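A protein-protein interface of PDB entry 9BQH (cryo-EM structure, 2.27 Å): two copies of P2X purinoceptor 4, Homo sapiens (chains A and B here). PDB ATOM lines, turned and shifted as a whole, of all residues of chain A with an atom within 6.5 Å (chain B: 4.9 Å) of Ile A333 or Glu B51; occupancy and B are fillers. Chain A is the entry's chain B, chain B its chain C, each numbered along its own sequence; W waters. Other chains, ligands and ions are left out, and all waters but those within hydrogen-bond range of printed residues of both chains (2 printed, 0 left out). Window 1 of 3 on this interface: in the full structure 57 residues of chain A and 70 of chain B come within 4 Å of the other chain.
O of Tyr B42 is in hydrogen-bond range of N of Val B47 (3.4 Å).
The backbone carbonyl oxygen of Trp B46 lies within hydrogen-bond range of the backbone NH of Glu B51 (2.8 Å).
OE2 of Glu B51 sits close to NE1 of Trp B50, at 3.4 Å.
Water W2 lies within hydrogen-bond range of OD1 of Asp A331 (2.6 Å) and NE1 of Trp B46 (3.2 Å).
Water W1 lies within hydrogen-bond range of the backbone carbonyl oxygen (O) of Ile A333 (3.0 Å) and the side-chain hydroxyl (OH) of Tyr B42 (3.1 Å).
Of the 10 printed residues of chain B, 3 touch a printed residue of chain A.
Along chain B the printed residues that touch a printed residue of chain A span positions 42 to 51.
Of the 10 printed residues of chain A, 3 touch a printed residue of chain B.
Among the printed residues, 5 pairs touch across the chains.
Among the printed residues, no Asp or Glu carboxylate lies within 4 Å of a Lys or Arg side-chain nitrogen of the other chain.
Among the printed residues, merely in contact across the chains: Met A336 with Tyr B42, Ile A332 with Tyr B42, Ile A333 with Tyr B42, Ile A333 with Glu B51 and Ile A332 with Trp B46.
Ile A333 touches just these residues of chain B: Tyr B42 (3.7 Å) and Glu B51 (3.8 Å).
Printed residues of chain A within 4 Å of Tyr B42: Ile A332, Ile A333 and Met A336.
Gly B45 touches none of the printed residues of chain A.
Printed residues of chain A within 4 Å of Trp B46: Ile A332 (3.8 Å).
Of chain A, only Ile A333 (3.8 Å) comes within 4 Å of Glu B51.
Position printed for both chains: 53.
Of the 5 pairs that touch across the chains among the printed residues, none has its exchanged pair printed and touching as well.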
ATOM      1  N   GLY A  53       8.571  -3.969  24.424  1.00  0.00           N
ATOM      2  CA  GLY A  53       9.172  -4.298  23.148  1.00  0.00           C
ATOM      3  C   GLY A  53       8.595  -3.553  21.968  1.00  0.00           C
ATOM      4  O   GLY A  53       9.056  -3.756  20.841  1.00  0.00           O
ATOM      5  N   GLU A  56      10.838   2.397  20.644  1.00  0.00           N
ATOM      6  CA  GLU A  56      12.195   2.811  20.326  1.00  0.00           C
ATOM      7  C   GLU A  56      12.740   3.674  21.462  1.00  0.00           C
ATOM      8  O   GLU A  56      11.988   4.296  22.213  1.00  0.00           O
ATOM      9  CB  GLU A  56      12.230   3.581  19.004  1.00  0.00           C
ATOM     10  CG  GLU A  56      11.884   5.060  19.130  1.00  0.00           C
ATOM     11  CD  GLU A  56      11.173   5.607  17.907  1.00  0.00           C
ATOM     12  OE1 GLU A  56      11.838   5.805  16.869  1.00  0.00           O
ATOM     13  OE2 GLU A  56       9.949   5.850  17.987  1.00  0.00           O
ATOM     14  N   ASP A 331       7.068   2.641  18.489  1.00  0.00           N
ATOM     15  CA  ASP A 331       7.539   2.573  17.116  1.00  0.00           C
ATOM     16  C   ASP A 331       7.005   1.300  16.477  1.00  0.00           C
ATOM     17  O   ASP A 331       6.833   0.279  17.145  1.00  0.00           O
ATOM     18  CB  ASP A 331       9.070   2.599  17.043  1.00  0.00           C
ATOM     19  CG  ASP A 331       9.585   2.973  15.665  1.00  0.00           C
ATOM     20  OD1 ASP A 331       8.778   3.415  14.823  1.00  0.00           O
ATOM     21  OD2 ASP A 331      10.799   2.829  15.423  1.00  0.00           O
ATOM     22  N   ILE A 332       6.743   1.370  15.172  1.00  0.00           N
ATOM     23  CA  ILE A 332       6.103   0.250  14.493  1.00  0.00           C
ATOM     24  C   ILE A 332       7.110  -0.841  14.136  1.00  0.00           C
ATOM     25  O   ILE A 332       6.740  -2.015  14.034  1.00  0.00           O
ATOM     26  CB  ILE A 332       5.348   0.750  13.249  1.00  0.00           C
ATOM     27  CG1 ILE A 332       4.430  -0.343  12.693  1.00  0.00           C
ATOM     28  CG2 ILE A 332       6.322   1.206  12.173  1.00  0.00           C
ATOM     29  CD1 ILE A 332       3.306  -0.741  13.619  1.00  0.00           C
ATOM     30  N   ILE A 333       8.378  -0.493  13.948  1.00  0.00           N
ATOM     31  CA  ILE A 333       9.387  -1.452  13.501  1.00  0.00           C
ATOM     32  C   ILE A 333       9.628  -2.509  14.576  1.00  0.00           C
ATOM     33  O   ILE A 333       9.534  -3.709  14.280  1.00  0.00           O
ATOM     34  CB  ILE A 333      10.687  -0.730  13.105  1.00  0.00           C
ATOM     35  CG1 ILE A 333      10.401   0.217  11.935  1.00  0.00           C
ATOM     36  CG2 ILE A 333      11.785  -1.736  12.746  1.00  0.00           C
ATOM     37  CD1 ILE A 333      11.580   0.504  11.040  1.00  0.00           C
ATOM     38  N   PRO A 334       9.970  -2.134  15.814  1.00  0.00           N
ATOM     39  CA  PRO A 334      10.105  -3.166  16.859  1.00  0.00           C
ATOM     40  C   PRO A 334       8.820  -3.937  17.108  1.00  0.00           C
ATOM     41  O   PRO A 334       8.862  -5.145  17.376  1.00  0.00           O
ATOM     42  CB  PRO A 334      10.545  -2.360  18.091  1.00  0.00           C
ATOM     43  CG  PRO A 334      10.195  -0.948  17.790  1.00  0.00           C
ATOM     44  CD  PRO A 334      10.343  -0.802  16.316  1.00  0.00           C
ATOM     45  N   THR A 335       7.669  -3.267  17.007  1.00  0.00           N
ATOM     46  CA  THR A 335       6.391  -3.946  17.185  1.00  0.00           C
ATOM     47  C   THR A 335       6.221  -5.068  16.168  1.00  0.00           C
ATOM     48  O   THR A 335       5.890  -6.206  16.526  1.00  0.00           O
ATOM     49  CB  THR A 335       5.249  -2.935  17.063  1.00  0.00           C
ATOM     50  OG1 THR A 335       5.462  -1.857  17.979  1.00  0.00           O
ATOM     51  CG2 THR A 335       3.908  -3.586  17.359  1.00  0.00           C
ATOM     52  N   MET A 336       6.458  -4.768  14.890  1.00  0.00           N
ATOM     53  CA  MET A 336       6.286  -5.782  13.859  1.00  0.00           C
ATOM     54  C   MET A 336       7.364  -6.850  13.937  1.00  0.00           C
ATOM     55  O   MET A 336       7.089  -8.019  13.648  1.00  0.00           O
ATOM     56  CB  MET A 336       6.278  -5.136  12.474  1.00  0.00           C
ATOM     57  CG  MET A 336       5.071  -4.249  12.186  1.00  0.00           C
ATOM     58  SD  MET A 336       3.508  -4.858  12.846  1.00  0.00           S
ATOM     59  CE  MET A 336       3.017  -5.998  11.562  1.00  0.00           C
ATOM     60  N   ILE A 337       8.585  -6.486  14.337  1.00  0.00           N
ATOM     61  CA  ILE A 337       9.623  -7.498  14.518  1.00  0.00           C
ATOM     62  C   ILE A 337       9.197  -8.500  15.582  1.00  0.00           C
ATOM     63  O   ILE A 337       9.330  -9.716  15.405  1.00  0.00           O
ATOM     64  CB  ILE A 337      10.970  -6.837  14.863  1.00  0.00           C
ATOM     65  CG1 ILE A 337      11.668  -6.365  13.588  1.00  0.00           C
ATOM     66  CG2 ILE A 337      11.868  -7.805  15.625  1.00  0.00           C
ATOM     67  CD1 ILE A 337      12.775  -5.368  13.831  1.00  0.00           C
ATOM     68  N   ASN A 338       8.662  -8.006  16.701  1.00  0.00           N
ATOM     69  CA  ASN A 338       8.242  -8.907  17.769  1.00  0.00           C
ATOM     70  C   ASN A 338       7.022  -9.728  17.365  1.00  0.00           C
ATOM     71  O   ASN A 338       6.916 -10.906  17.722  1.00  0.00           O
ATOM     72  CB  ASN A 338       7.964  -8.111  19.041  1.00  0.00           C
ATOM     73  CG  ASN A 338       9.233  -7.685  19.747  1.00  0.00           C
ATOM     74  OD1 ASN A 338       9.428  -6.508  20.039  1.00  0.00           O
ATOM     75  ND2 ASN A 338      10.106  -8.643  20.029  1.00  0.00           N
ATOM     76  N   TYR B  42       5.501  -2.590   3.016  1.00  0.00           N
ATOM     77  CA  TYR B  42       5.997  -2.217   4.333  1.00  0.00           C
ATOM     78  C   TYR B  42       7.450  -2.647   4.498  1.00  0.00           C
ATOM     79  O   TYR B  42       8.351  -1.811   4.634  1.00  0.00           O
ATOM     80  CB  TYR B  42       5.124  -2.840   5.423  1.00  0.00           C
ATOM     81  CG  TYR B  42       5.720  -2.711   6.803  1.00  0.00           C
ATOM     82  CD1 TYR B  42       5.724  -1.494   7.467  1.00  0.00           C
ATOM     83  CD2 TYR B  42       6.296  -3.802   7.435  1.00  0.00           C
ATOM     84  CE1 TYR B  42       6.273  -1.370   8.724  1.00  0.00           C
ATOM     85  CE2 TYR B  42       6.851  -3.688   8.690  1.00  0.00           C
ATOM     86  CZ  TYR B  42       6.836  -2.469   9.330  1.00  0.00           C
ATOM     87  OH  TYR B  42       7.389  -2.351  10.581  1.00  0.00           O
ATOM     88  N   GLY B  45       9.910  -0.836   1.633  1.00  0.00           N
ATOM     89  CA  GLY B  45       9.982   0.614   1.607  1.00  0.00           C
ATOM     90  C   GLY B  45      10.257   1.222   2.968  1.00  0.00           C
ATOM     91  O   GLY B  45      11.134   2.077   3.108  1.00  0.00           O
ATOM     92  N   TRP B  46       9.512   0.801   3.991  1.00  0.00           N
ATOM     93  CA  TRP B  46       9.649   1.458   5.282  1.00  0.00           C
ATOM     94  C   TRP B  46      10.862   0.938   6.044  1.00  0.00           C
ATOM     95  O   TRP B  46      11.712   1.718   6.481  1.00  0.00           O
ATOM     96  CB  TRP B  46       8.379   1.268   6.109  1.00  0.00           C
ATOM     97  CG  TRP B  46       8.367   2.108   7.340  1.00  0.00           C
ATOM     98  CD1 TRP B  46       8.515   1.683   8.624  1.00  0.00           C
ATOM     99  CD2 TRP B  46       8.209   3.529   7.403  1.00  0.00           C
ATOM    100  NE1 TRP B  46       8.455   2.749   9.486  1.00  0.00           N
ATOM    101  CE2 TRP B  46       8.269   3.895   8.761  1.00  0.00           C
ATOM    102  CE3 TRP B  46       8.022   4.528   6.443  1.00  0.00           C
ATOM    103  CZ2 TRP B  46       8.147   5.216   9.180  1.00  0.00           C
ATOM    104  CZ3 TRP B  46       7.900   5.836   6.863  1.00  0.00           C
ATOM    105  CH2 TRP B  46       7.964   6.170   8.220  1.00  0.00           C
ATOM    106  N   VAL B  47      10.960  -0.381   6.209  1.00  0.00           N
ATOM    107  CA  VAL B  47      12.010  -0.940   7.054  1.00  0.00           C
ATOM    108  C   VAL B  47      13.374  -0.789   6.389  1.00  0.00           C
ATOM    109  O   VAL B  47      14.350  -0.393   7.036  1.00  0.00           O
ATOM    110  CB  VAL B  47      11.699  -2.408   7.392  1.00  0.00           C
ATOM    111  CG1 VAL B  47      12.864  -3.042   8.131  1.00  0.00           C
ATOM    112  CG2 VAL B  47      10.429  -2.503   8.213  1.00  0.00           C
ATOM    113  N   PHE B  48      13.471  -1.101   5.096  1.00  0.00           N
ATOM    114  CA  PHE B  48      14.773  -1.129   4.437  1.00  0.00           C
ATOM    115  C   PHE B  48      15.108   0.211   3.784  1.00  0.00           C
ATOM    116  O   PHE B  48      16.112   0.841   4.124  1.00  0.00           O
ATOM    117  CB  PHE B  48      14.812  -2.252   3.392  1.00  0.00           C
ATOM    118  CG  PHE B  48      15.111  -3.610   3.963  1.00  0.00           C
ATOM    119  CD1 PHE B  48      16.231  -3.821   4.746  1.00  0.00           C
ATOM    120  CD2 PHE B  48      14.272  -4.680   3.706  1.00  0.00           C
ATOM    121  CE1 PHE B  48      16.503  -5.071   5.267  1.00  0.00           C
ATOM    122  CE2 PHE B  48      14.541  -5.930   4.226  1.00  0.00           C
ATOM    123  CZ  PHE B  48      15.657  -6.125   5.005  1.00  0.00           C
ATOM    124  N   VAL B  49      14.273   0.658   2.846  1.00  0.00           N
ATOM    125  CA  VAL B  49      14.615   1.836   2.054  1.00  0.00           C
ATOM    126  C   VAL B  49      14.552   3.099   2.905  1.00  0.00           C
ATOM    127  O   VAL B  49      15.445   3.951   2.845  1.00  0.00           O
ATOM    128  CB  VAL B  49      13.695   1.940   0.824  1.00  0.00           C
ATOM    129  CG1 VAL B  49      13.790   3.319   0.202  1.00  0.00           C
ATOM    130  CG2 VAL B  49      14.050   0.870  -0.190  1.00  0.00           C
ATOM    131  N   TRP B  50      13.500   3.240   3.711  1.00  0.00           N
ATOM    132  CA  TRP B  50      13.274   4.495   4.421  1.00  0.00           C
ATOM    133  C   TRP B  50      14.057   4.553   5.727  1.00  0.00           C
ATOM    134  O   TRP B  50      14.830   5.488   5.959  1.00  0.00           O
ATOM    135  CB  TRP B  50      11.778   4.680   4.689  1.00  0.00           C
ATOM    136  CG  TRP B  50      11.440   6.027   5.239  1.00  0.00           C
ATOM    137  CD1 TRP B  50      11.373   6.384   6.552  1.00  0.00           C
ATOM    138  CD2 TRP B  50      11.120   7.203   4.487  1.00  0.00           C
ATOM    139  NE1 TRP B  50      11.034   7.709   6.667  1.00  0.00           N
ATOM    140  CE2 TRP B  50      10.870   8.234   5.413  1.00  0.00           C
ATOM    141  CE3 TRP B  50      11.019   7.483   3.122  1.00  0.00           C
ATOM    142  CZ2 TRP B  50      10.529   9.523   5.018  1.00  0.00           C
ATOM    143  CZ3 TRP B  50      10.678   8.765   2.733  1.00  0.00           C
ATOM    144  CH2 TRP B  50      10.437   9.768   3.677  1.00  0.00           C
ATOM    145  N   GLU B  51      13.867   3.565   6.596  1.00  0.00           N
ATOM    146  CA  GLU B  51      14.467   3.575   7.923  1.00  0.00           C
ATOM    147  C   GLU B  51      15.806   2.854   7.982  1.00  0.00           C
ATOM    148  O   GLU B  51      16.405   2.787   9.060  1.00  0.00           O
ATOM    149  CB  GLU B  51      13.502   2.954   8.934  1.00  0.00           C
ATOM    150  CG  GLU B  51      12.206   3.726   9.087  1.00  0.00           C
ATOM    151  CD  GLU B  51      12.359   4.950   9.963  1.00  0.00           C
ATOM    152  OE1 GLU B  51      12.892   4.818  11.084  1.00  0.00           O
ATOM    153  OE2 GLU B  51      11.951   6.047   9.528  1.00  0.00           O
ATOM    154  N   LYS B  52      16.290   2.318   6.862  1.00  0.00           N
ATOM    155  CA  LYS B  52      17.604   1.681   6.789  1.00  0.00           C
ATOM    156  C   LYS B  52      17.735   0.572   7.834  1.00  0.00           C
ATOM    157  O   LYS B  52      18.612   0.593   8.699  1.00  0.00           O
ATOM    158  CB  LYS B  52      18.718   2.720   6.946  1.00  0.00           C
ATOM    159  CG  LYS B  52      18.505   3.979   6.129  1.00  0.00           C
ATOM    160  CD  LYS B  52      19.752   4.371   5.359  1.00  0.00           C
ATOM    161  CE  LYS B  52      19.440   5.361   4.246  1.00  0.00           C
ATOM    162  NZ  LYS B  52      18.367   4.886   3.328  1.00  0.00           N
ATOM    163  N   GLY B  53      16.846  -0.411   7.729  1.00  0.00           N
ATOM    164  CA  GLY B  53      16.876  -1.558   8.612  1.00  0.00           C
ATOM    165  C   GLY B  53      17.987  -2.542   8.333  1.00  0.00           C
ATOM    166  O   GLY B  53      18.102  -3.543   9.045  1.00  0.00           O
HETATM  167  O   HOH W   1       9.543  -4.381  11.400  1.00  0.00           O
HETATM  168  O   HOH W   2       9.436   3.838  12.363  1.00  0.00           O
